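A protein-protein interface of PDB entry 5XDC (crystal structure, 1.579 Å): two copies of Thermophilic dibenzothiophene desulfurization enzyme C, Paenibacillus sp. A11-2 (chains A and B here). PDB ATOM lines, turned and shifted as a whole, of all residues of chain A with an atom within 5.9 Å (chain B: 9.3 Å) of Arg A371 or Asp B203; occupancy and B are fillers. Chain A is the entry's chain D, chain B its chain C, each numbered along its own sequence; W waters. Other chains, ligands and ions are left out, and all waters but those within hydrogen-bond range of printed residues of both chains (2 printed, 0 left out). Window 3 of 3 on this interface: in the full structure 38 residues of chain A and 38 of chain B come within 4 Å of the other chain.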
ATOM      1  N   ARG A  37       5.194 -18.250  10.453  1.00  0.00           N
ATOM      2  CA  ARG A  37       3.892 -17.909   9.882  1.00  0.00           C
ATOM      3  C   ARG A  37       4.005 -16.729   8.932  1.00  0.00           C
ATOM      4  O   ARG A  37       3.413 -16.729   7.846  1.00  0.00           O
ATOM      5  CB  ARG A  37       2.900 -17.583  10.993  1.00  0.00           C
ATOM      6  CG  ARG A  37       2.322 -18.782  11.680  1.00  0.00           C
ATOM      7  CD  ARG A  37       1.209 -18.356  12.624  1.00  0.00           C
ATOM      8  NE  ARG A  37       1.296 -19.049  13.904  1.00  0.00           N
ATOM      9  CZ  ARG A  37       0.452 -18.871  14.915  1.00  0.00           C
ATOM     10  NH1 ARG A  37      -0.562 -18.017  14.804  1.00  0.00           N
ATOM     11  NH2 ARG A  37       0.624 -19.553  16.040  1.00  0.00           N
ATOM     12  N   ALA A 367      -3.750 -31.817  20.088  1.00  0.00           N
ATOM     13  CA  ALA A 367      -2.566 -31.295  19.421  1.00  0.00           C
ATOM     14  C   ALA A 367      -2.849 -30.817  18.010  1.00  0.00           C
ATOM     15  O   ALA A 367      -2.093 -29.989  17.499  1.00  0.00           O
ATOM     16  CB  ALA A 367      -1.475 -32.358  19.381  1.00  0.00           C
ATOM     17  N   ALA A 368      -3.889 -31.344  17.358  1.00  0.00           N
ATOM     18  CA  ALA A 368      -4.345 -30.863  16.064  1.00  0.00           C
ATOM     19  C   ALA A 368      -5.519 -29.903  16.171  1.00  0.00           C
ATOM     20  O   ALA A 368      -5.682 -29.030  15.309  1.00  0.00           O
ATOM     21  CB  ALA A 368      -4.751 -32.046  15.185  1.00  0.00           C
ATOM     22  N   ALA A 369      -6.333 -30.039  17.214  1.00  0.00           N
ATOM     23  CA  ALA A 369      -7.498 -29.173  17.357  1.00  0.00           C
ATOM     24  C   ALA A 369      -7.091 -27.731  17.615  1.00  0.00           C
ATOM     25  O   ALA A 369      -7.830 -26.802  17.269  1.00  0.00           O
ATOM     26  CB  ALA A 369      -8.384 -29.680  18.489  1.00  0.00           C
ATOM     27  N   SER A 370      -5.926 -27.527  18.206  1.00  0.00           N
ATOM     28  CA  SER A 370      -5.403 -26.199  18.500  1.00  0.00           C
ATOM     29  C   SER A 370      -4.341 -25.860  17.467  1.00  0.00           C
ATOM     30  O   SER A 370      -3.179 -26.253  17.605  1.00  0.00           O
ATOM     31  CB  SER A 370      -4.822 -26.143  19.906  1.00  0.00           C
ATOM     32  OG  SER A 370      -4.042 -24.962  20.062  1.00  0.00           O
ATOM     33  N   ARG A 371      -4.740 -25.112  16.434  1.00  0.00           N
ATOM     34  CA  ARG A 371      -3.797 -24.754  15.378  1.00  0.00           C
ATOM     35  C   ARG A 371      -2.587 -24.019  15.938  1.00  0.00           C
ATOM     36  O   ARG A 371      -1.479 -24.156  15.407  1.00  0.00           O
ATOM     37  CB  ARG A 371      -4.487 -23.889  14.323  1.00  0.00           C
ATOM     38  CG  ARG A 371      -3.596 -23.524  13.131  1.00  0.00           C
ATOM     39  CD  ARG A 371      -4.253 -22.499  12.199  1.00  0.00           C
ATOM     40  NE  ARG A 371      -4.761 -21.345  12.935  1.00  0.00           N
ATOM     41  CZ  ARG A 371      -4.001 -20.368  13.426  1.00  0.00           C
ATOM     42  NH1 ARG A 371      -2.681 -20.381  13.260  1.00  0.00           N
ATOM     43  NH2 ARG A 371      -4.565 -19.369  14.089  1.00  0.00           N
ATOM     44  N   GLN A 372      -2.779 -23.256  17.019  1.00  0.00           N
ATOM     45  CA  GLN A 372      -1.700 -22.445  17.579  1.00  0.00           C
ATOM     46  C   GLN A 372      -0.532 -23.276  18.097  1.00  0.00           C
ATOM     47  O   GLN A 372       0.593 -22.771  18.181  1.00  0.00           O
ATOM     48  CB  GLN A 372      -2.249 -21.576  18.712  1.00  0.00           C
ATOM     49  N   PHE A 373      -0.776 -24.523  18.503  1.00  0.00           N
ATOM     50  CA  PHE A 373       0.319 -25.371  18.948  1.00  0.00           C
ATOM     51  C   PHE A 373       1.404 -25.432  17.880  1.00  0.00           C
ATOM     52  O   PHE A 373       2.601 -25.445  18.190  1.00  0.00           O
ATOM     53  CB  PHE A 373      -0.227 -26.766  19.283  1.00  0.00           C
ATOM     54  CG  PHE A 373       0.816 -27.751  19.696  1.00  0.00           C
ATOM     55  CD1 PHE A 373       1.860 -27.375  20.525  1.00  0.00           C
ATOM     56  CD2 PHE A 373       0.738 -29.068  19.285  1.00  0.00           C
ATOM     57  CE1 PHE A 373       2.813 -28.281  20.917  1.00  0.00           C
ATOM     58  CE2 PHE A 373       1.700 -29.990  19.681  1.00  0.00           C
ATOM     59  CZ  PHE A 373       2.741 -29.586  20.491  1.00  0.00           C
ATOM     60  N   GLY A 374       0.999 -25.486  16.616  1.00  0.00           N
ATOM     61  CA  GLY A 374       1.928 -25.319  15.513  1.00  0.00           C
ATOM     62  C   GLY A 374       2.847 -26.490  15.239  1.00  0.00           C
ATOM     63  O   GLY A 374       3.861 -26.312  14.558  1.00  0.00           O
ATOM     64  N   PHE A 375       2.521 -27.684  15.722  1.00  0.00           N
ATOM     65  CA  PHE A 375       3.404 -28.827  15.526  1.00  0.00           C
ATOM     66  C   PHE A 375       3.523 -29.229  14.063  1.00  0.00           C
ATOM     67  O   PHE A 375       4.515 -29.878  13.693  1.00  0.00           O
ATOM     68  CB  PHE A 375       2.904 -30.020  16.338  1.00  0.00           C
ATOM     69  CG  PHE A 375       3.829 -31.196  16.320  1.00  0.00           C
ATOM     70  CD1 PHE A 375       4.898 -31.275  17.201  1.00  0.00           C
ATOM     71  CD2 PHE A 375       3.611 -32.238  15.436  1.00  0.00           C
ATOM     72  CE1 PHE A 375       5.748 -32.373  17.193  1.00  0.00           C
ATOM     73  CE2 PHE A 375       4.444 -33.330  15.422  1.00  0.00           C
ATOM     74  CZ  PHE A 375       5.510 -33.403  16.307  1.00  0.00           C
ATOM     75  N   ASP A 376       2.549 -28.860  13.229  1.00  0.00           N
ATOM     76  CA  ASP A 376       2.586 -29.221  11.818  1.00  0.00           C
ATOM     77  C   ASP A 376       3.750 -28.564  11.087  1.00  0.00           C
ATOM     78  O   ASP A 376       4.080 -28.980   9.974  1.00  0.00           O
ATOM     79  CB  ASP A 376       1.255 -28.856  11.139  1.00  0.00           C
ATOM     80  CG  ASP A 376       0.957 -27.375  11.202  1.00  0.00           C
ATOM     81  OD1 ASP A 376       0.830 -26.858  12.333  1.00  0.00           O
ATOM     82  OD2 ASP A 376       0.888 -26.735  10.131  1.00  0.00           O
ATOM     83  N   GLU B  36     -11.649 -22.536   3.464  1.00  0.00           N
ATOM     84  CA  GLU B  36     -11.160 -23.151   4.697  1.00  0.00           C
ATOM     85  C   GLU B  36      -9.987 -22.398   5.307  1.00  0.00           C
ATOM     86  O   GLU B  36      -9.766 -22.504   6.519  1.00  0.00           O
ATOM     87  CB  GLU B  36     -10.795 -24.625   4.487  1.00  0.00           C
ATOM     88  CG  GLU B  36      -9.522 -24.888   3.760  1.00  0.00           C
ATOM     89  CD  GLU B  36      -8.297 -25.056   4.662  1.00  0.00           C
ATOM     90  OE1 GLU B  36      -8.342 -25.679   5.763  1.00  0.00           O
ATOM     91  OE2 GLU B  36      -7.253 -24.551   4.244  1.00  0.00           O
ATOM     92  N   ARG B  37      -9.251 -21.620   4.518  1.00  0.00           N
ATOM     93  CA  ARG B  37      -8.223 -20.759   5.097  1.00  0.00           C
ATOM     94  C   ARG B  37      -8.807 -19.854   6.181  1.00  0.00           C
ATOM     95  O   ARG B  37      -8.217 -19.685   7.253  1.00  0.00           O
ATOM     96  CB  ARG B  37      -7.567 -19.929   3.991  1.00  0.00           C
ATOM     97  N   ALA B  38      -9.991 -19.294   5.936  1.00  0.00           N
ATOM     98  CA  ALA B  38     -10.599 -18.382   6.895  1.00  0.00           C
ATOM     99  C   ALA B  38     -11.177 -19.094   8.111  1.00  0.00           C
ATOM    100  O   ALA B  38     -11.327 -18.472   9.168  1.00  0.00           O
ATOM    101  CB  ALA B  38     -11.696 -17.577   6.211  1.00  0.00           C
ATOM    102  N   GLY B  39     -11.495 -20.374   7.999  1.00  0.00           N
ATOM    103  CA  GLY B  39     -12.139 -21.017   9.124  1.00  0.00           C
ATOM    104  C   GLY B  39     -13.553 -20.477   9.238  1.00  0.00           C
ATOM    105  O   GLY B  39     -14.144 -19.984   8.272  1.00  0.00           O
ATOM    106  N   GLY B  40     -14.094 -20.563  10.436  1.00  0.00           N
ATOM    107  CA  GLY B  40     -15.438 -20.040  10.617  1.00  0.00           C
ATOM    108  C   GLY B  40     -16.499 -20.930   9.982  1.00  0.00           C
ATOM    109  O   GLY B  40     -16.264 -22.084   9.595  1.00  0.00           O
ATOM    110  N   GLY B 200     -17.447 -20.096  19.834  1.00  0.00           N
ATOM    111  CA  GLY B 200     -16.739 -19.681  18.629  1.00  0.00           C
ATOM    112  C   GLY B 200     -15.230 -19.701  18.755  1.00  0.00           C
ATOM    113  O   GLY B 200     -14.553 -18.813  18.218  1.00  0.00           O
ATOM    114  N   ASP B 201     -14.678 -20.711  19.429  1.00  0.00           N
ATOM    115  CA  ASP B 201     -13.243 -20.795  19.670  1.00  0.00           C
ATOM    116  C   ASP B 201     -12.564 -21.921  18.883  1.00  0.00           C
ATOM    117  O   ASP B 201     -11.476 -22.364  19.257  1.00  0.00           O
ATOM    118  CB  ASP B 201     -12.973 -20.961  21.164  1.00  0.00           C
ATOM    119  CG  ASP B 201     -13.758 -22.105  21.788  1.00  0.00           C
ATOM    120  OD1 ASP B 201     -14.470 -22.817  21.059  1.00  0.00           O
ATOM    121  OD2 ASP B 201     -13.625 -22.303  23.008  1.00  0.00           O
ATOM    122  N   TRP B 202     -13.161 -22.370  17.790  1.00  0.00           N
ATOM    123  CA  TRP B 202     -12.570 -23.436  16.986  1.00  0.00           C
ATOM    124  C   TRP B 202     -11.577 -22.837  16.000  1.00  0.00           C
ATOM    125  O   TRP B 202     -11.957 -22.082  15.102  1.00  0.00           O
ATOM    126  CB  TRP B 202     -13.656 -24.197  16.242  1.00  0.00           C
ATOM    127  CG  TRP B 202     -13.191 -25.323  15.362  1.00  0.00           C
ATOM    128  CD1 TRP B 202     -13.274 -25.380  14.002  1.00  0.00           C
ATOM    129  CD2 TRP B 202     -12.615 -26.568  15.779  1.00  0.00           C
ATOM    130  NE1 TRP B 202     -12.783 -26.580  13.542  1.00  0.00           N
ATOM    131  CE2 TRP B 202     -12.376 -27.329  14.612  1.00  0.00           C
ATOM    132  CE3 TRP B 202     -12.291 -27.115  17.016  1.00  0.00           C
ATOM    133  CZ2 TRP B 202     -11.820 -28.606  14.655  1.00  0.00           C
ATOM    134  CZ3 TRP B 202     -11.731 -28.376  17.052  1.00  0.00           C
ATOM    135  CH2 TRP B 202     -11.500 -29.105  15.880  1.00  0.00           C
ATOM    136  N   ASP B 203     -10.305 -23.187  16.164  1.00  0.00           N
ATOM    137  CA  ASP B 203      -9.247 -22.707  15.279  1.00  0.00           C
ATOM    138  C   ASP B 203      -8.221 -23.842  15.186  1.00  0.00           C
ATOM    139  O   ASP B 203      -7.325 -23.956  16.023  1.00  0.00           O
ATOM    140  CB  ASP B 203      -8.650 -21.422  15.833  1.00  0.00           C
ATOM    141  CG  ASP B 203      -7.451 -20.950  15.049  1.00  0.00           C
ATOM    142  OD1 ASP B 203      -7.403 -21.188  13.823  1.00  0.00           O
ATOM    143  OD2 ASP B 203      -6.563 -20.338  15.672  1.00  0.00           O
ATOM    144  N   SER B 204      -8.398 -24.696  14.182  1.00  0.00           N
ATOM    145  CA  SER B 204      -7.806 -26.024  14.165  1.00  0.00           C
ATOM    146  C   SER B 204      -6.832 -26.193  13.002  1.00  0.00           C
ATOM    147  O   SER B 204      -6.823 -25.413  12.044  1.00  0.00           O
ATOM    148  CB  SER B 204      -8.904 -27.073  14.054  1.00  0.00           C
ATOM    149  OG  SER B 204      -9.651 -26.840  12.878  1.00  0.00           O
ATOM    150  N   LEU B 205      -6.017 -27.251  13.083  1.00  0.00           N
ATOM    151  CA  LEU B 205      -5.109 -27.571  11.981  1.00  0.00           C
ATOM    152  C   LEU B 205      -5.878 -27.878  10.704  1.00  0.00           C
ATOM    153  O   LEU B 205      -5.613 -27.294   9.648  1.00  0.00           O
ATOM    154  CB  LEU B 205      -4.223 -28.750  12.367  1.00  0.00           C
ATOM    155  CG  LEU B 205      -3.302 -29.288  11.279  1.00  0.00           C
ATOM    156  CD1 LEU B 205      -2.236 -28.270  10.906  1.00  0.00           C
ATOM    157  CD2 LEU B 205      -2.671 -30.571  11.767  1.00  0.00           C
ATOM    158  N   GLY B 206      -6.838 -28.803  10.786  1.00  0.00           N
ATOM    159  CA  GLY B 206      -7.716 -29.163   9.694  1.00  0.00           C
ATOM    160  C   GLY B 206      -9.152 -29.264  10.187  1.00  0.00           C
ATOM    161  O   GLY B 206      -9.406 -28.979  11.358  1.00  0.00           O
ATOM    162  N   MET B 207     -10.079 -29.681   9.327  1.00  0.00           N
ATOM    163  CA  MET B 207     -11.506 -29.632   9.649  1.00  0.00           C
ATOM    164  C   MET B 207     -11.883 -28.228  10.105  1.00  0.00           C
ATOM    165  O   MET B 207     -12.691 -28.034  11.019  1.00  0.00           O
ATOM    166  CB  MET B 207     -11.863 -30.685  10.701  1.00  0.00           C
ATOM    167  CG  MET B 207     -11.719 -32.117  10.184  1.00  0.00           C
ATOM    168  SD  MET B 207     -12.712 -32.394   8.693  1.00  0.00           S
ATOM    169  CE  MET B 207     -12.561 -34.167   8.497  1.00  0.00           C
ATOM    170  N   ARG B 208     -11.306 -27.230   9.427  1.00  0.00           N
ATOM    171  CA  ARG B 208     -11.340 -25.866   9.935  1.00  0.00           C
ATOM    172  C   ARG B 208     -12.726 -25.227   9.884  1.00  0.00           C
ATOM    173  O   ARG B 208     -12.943 -24.235  10.581  1.00  0.00           O
ATOM    174  CB  ARG B 208     -10.342 -24.996   9.166  1.00  0.00           C
ATOM    175  CG  ARG B 208      -8.905 -25.284   9.561  1.00  0.00           C
ATOM    176  CD  ARG B 208      -7.906 -24.338   8.914  1.00  0.00           C
ATOM    177  NE  ARG B 208      -8.259 -22.928   9.063  1.00  0.00           N
ATOM    178  CZ  ARG B 208      -8.087 -22.212  10.170  1.00  0.00           C
ATOM    179  NH1 ARG B 208      -7.586 -22.764  11.268  1.00  0.00           N
ATOM    180  NH2 ARG B 208      -8.433 -20.922  10.180  1.00  0.00           N
ATOM    181  N   GLN B 209     -13.662 -25.756   9.103  1.00  0.00           N
ATOM    182  CA  GLN B 209     -14.991 -25.153   8.986  1.00  0.00           C
ATOM    183  C   GLN B 209     -16.079 -26.023   9.620  1.00  0.00           C
ATOM    184  O   GLN B 209     -17.258 -25.931   9.254  1.00  0.00           O
ATOM    185  CB  GLN B 209     -15.314 -24.862   7.524  1.00  0.00           C
ATOM    186  CG  GLN B 209     -14.490 -23.708   6.944  1.00  0.00           C
ATOM    187  CD  GLN B 209     -15.152 -23.033   5.759  1.00  0.00           C
ATOM    188  OE1 GLN B 209     -15.282 -23.613   4.690  1.00  0.00           O
ATOM    189  NE2 GLN B 209     -15.588 -21.791   5.957  1.00  0.00           N
ATOM    190  N   THR B 210     -15.702 -26.852  10.590  1.00  0.00           N
ATOM    191  CA  THR B 210     -16.654 -27.734  11.261  1.00  0.00           C
ATOM    192  C   THR B 210     -17.209 -27.144  12.545  1.00  0.00           C
ATOM    193  O   THR B 210     -18.056 -27.784  13.179  1.00  0.00           O
ATOM    194  CB  THR B 210     -16.014 -29.091  11.583  1.00  0.00           C
ATOM    195  OG1 THR B 210     -14.945 -28.926  12.514  1.00  0.00           O
ATOM    196  CG2 THR B 210     -15.537 -29.794  10.299  1.00  0.00           C
ATOM    197  N   ASP B 211     -16.747 -25.963  12.962  1.00  0.00           N
ATOM    198  CA  ASP B 211     -17.242 -25.302  14.171  1.00  0.00           C
ATOM    199  C   ASP B 211     -17.315 -26.274  15.345  1.00  0.00           C
ATOM    200  O   ASP B 211     -18.343 -26.421  16.014  1.00  0.00           O
ATOM    201  CB  ASP B 211     -18.600 -24.650  13.911  1.00  0.00           C
ATOM    202  CG  ASP B 211     -18.486 -23.396  13.048  1.00  0.00           C
ATOM    203  OD1 ASP B 211     -17.865 -22.430  13.523  1.00  0.00           O
ATOM    204  OD2 ASP B 211     -19.016 -23.405  11.915  1.00  0.00           O
ATOM    205  N   SER B 212     -16.200 -26.952  15.604  1.00  0.00           N
ATOM    206  CA  SER B 212     -16.135 -27.966  16.651  1.00  0.00           C
ATOM    207  C   SER B 212     -15.581 -27.411  17.951  1.00  0.00           C
ATOM    208  O   SER B 212     -14.887 -28.119  18.693  1.00  0.00           O
ATOM    209  CB  SER B 212     -15.302 -29.158  16.180  1.00  0.00           C
ATOM    210  OG  SER B 212     -15.932 -29.770  15.089  1.00  0.00           O
ATOM    211  N   GLY B 213     -15.883 -26.153  18.250  1.00  0.00           N
ATOM    212  CA  GLY B 213     -15.403 -25.520  19.459  1.00  0.00           C
ATOM    213  C   GLY B 213     -16.233 -25.880  20.676  1.00  0.00           C
ATOM    214  O   GLY B 213     -16.997 -26.850  20.689  1.00  0.00           O
ATOM    215  N   SER B 214     -16.070 -25.070  21.719  1.00  0.00           N
ATOM    216  CA  SER B 214     -16.736 -25.307  22.990  1.00  0.00           C
ATOM    217  C   SER B 214     -18.106 -24.617  23.039  1.00  0.00           C
ATOM    218  O   SER B 214     -18.386 -23.646  22.324  1.00  0.00           O
ATOM    219  CB  SER B 214     -15.855 -24.833  24.148  1.00  0.00           C
ATOM    220  OG  SER B 214     -15.743 -23.420  24.145  1.00  0.00           O
ATOM    221  N   ARG B 380      -3.962 -32.124   6.438  1.00  0.00           N
ATOM    222  CA  ARG B 380      -4.388 -31.425   7.648  1.00  0.00           C
ATOM    223  C   ARG B 380      -5.752 -31.920   8.120  1.00  0.00           C
ATOM    224  O   ARG B 380      -5.948 -32.170   9.320  1.00  0.00           O
ATOM    225  CB  ARG B 380      -4.418 -29.913   7.416  1.00  0.00           C
ATOM    226  CG  ARG B 380      -3.042 -29.289   7.386  1.00  0.00           C
ATOM    227  CD  ARG B 380      -3.072 -27.767   7.354  1.00  0.00           C
ATOM    228  NE  ARG B 380      -3.495 -27.220   6.066  1.00  0.00           N
ATOM    229  CZ  ARG B 380      -4.703 -26.727   5.804  1.00  0.00           C
ATOM    230  NH1 ARG B 380      -5.645 -26.715   6.741  1.00  0.00           N
ATOM    231  NH2 ARG B 380      -4.972 -26.229   4.605  1.00  0.00           N
ATOM    232  N   THR B 384      -6.158 -34.320  11.501  1.00  0.00           N
ATOM    233  CA  THR B 384      -6.972 -33.803  12.602  1.00  0.00           C
ATOM    234  C   THR B 384      -8.029 -34.811  13.032  1.00  0.00           C
ATOM    235  O   THR B 384      -8.053 -35.235  14.190  1.00  0.00           O
ATOM    236  CB  THR B 384      -7.610 -32.459  12.208  1.00  0.00           C
ATOM    237  OG1 THR B 384      -6.579 -31.497  11.975  1.00  0.00           O
ATOM    238  CG2 THR B 384      -8.488 -31.907  13.306  1.00  0.00           C
HETATM  239  O   HOH W   1      -5.319 -22.315  17.884  1.00  0.00           O
HETATM  240  O   HOH W   2      -9.488 -24.899  18.221  1.00  0.00           O
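Hydrophobic or aromatic side chains of chain A within 4 Å of the printed part of chain B: Ala A368 and Ala A369. Of the 22 printed residues of chain B, 6 touch a printed residue of chain A. Printed residues of chain B that touch a printed residue of chain A: Trp B202, Asp B203, Ser B204, Leu B205, Arg B208 and Thr B384. Along chain B the printed residues that touch a printed residue of chain A span positions 202 to 384. Among the printed residues, 12 pairs touch across the chains. Among the printed residues, Asp or Glu carboxylates within 4 Å of a Lys or Arg side-chain nitrogen of the other chain: Arg A371 with Asp B203 (2.7 Å).
The backbone carbonyl oxygen (O) of Arg B37 lies within hydrogen-bond range of the guanidinium group (NH2) of Arg B208, at 3.2 Å. NE1 of Trp B202 sits at hydrogen-bond distance from O of Met B207 (2.9 Å). The side-chain hydroxyl of Thr B210 sits at hydrogen-bond distance from the indole nitrogen of Trp B202, 3.4 Å away. The backbone carbonyl oxygen (O) of Ser B204 lies within hydrogen-bond range of the guanidinium group (NH1) of Arg B208 (2.9 Å). The side-chain hydroxyl of Thr B384 lies within hydrogen-bond range of the backbone NH of Gly B206 (3.0 Å). The side-chain hydroxyl (OG1) of Thr B384 lies within hydrogen-bond range of the backbone carbonyl oxygen (O) of Arg B380 (2.8 Å).
Among the printed residues, pairs that only touch across the chains: Ala A369 with Ser B204 (3.2 Å), Asp A376 with Leu B205 (3.3 Å), Arg A371 with Arg B208 (3.5 Å), Arg A371 with Ser B204 (3.5 Å), Ala A368 with Thr B384 (3.7 Å), Ser A370 with Asp B203 (3.8 Å), Ala A368 with Ser B204 (3.8 Å), Ala A369 with Trp B202 (3.9 Å) and Arg A371 with Leu B205 (3.9 Å).
Water W2 lies within hydrogen-bond range of O of Ala A369 (2.7 Å), N of Asp B203 (2.8 Å) and O of Asp B201 (3.4 Å). Water W1 lies within hydrogen-bond range of N of Gln A372 (2.8 Å), O of Asp B203 (3.2 Å) and N of Arg A371 (3.2 Å).
Of the printed residues of chain B, Arg A371 touches Asp B203 (2.7 Å), Ser B204 (3.5 Å), Leu B205 (3.9 Å) and Arg B208 (3.5 Å). Printed residues of chain A within 4 Å of Asp B203: Ala A369, Ser A370 and Arg A371. Of chain B, only Asp B203 (3.8 Å) comes within 4 Å of Ser A370. No residue of chain B comes within 4 Å of Gln A372. Printed residues of chain A within 4 Å of Trp B202: Ala A369. Of the printed residues of chain A, Ser B204 touches Ala A368, Ala A369 and Arg A371. Of the printed residues of chain A, Leu B205 touches Ala A368, Arg A371 and Asp A376. Of the printed residues of chain A, Arg B208 touches Arg A371 (3.5 Å). Ala A367 touches none of the printed residues of chain B. Gln B209 touches none of the printed residues of chain A. The nearest printed residue of chain A that does not touch Thr B384 is Ala A369 (4.8 Å).
1 position is printed for both chains. Of the 12 pairs that touch across the chains among the printed residues, none has its exchanged pair printed and touching as well.
OD2 of Asp B203 lies within salt-bridge range of NH2 of Arg A371, at 2.7 Å. N of Leu B205 is in hydrogen-bond range of O of Ala A368, at 2.9 Å. The backbone carbonyl oxygen of Ala A369 lies close to the backbone carbonyl oxygen of Asp B203, 3.1 Å away.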
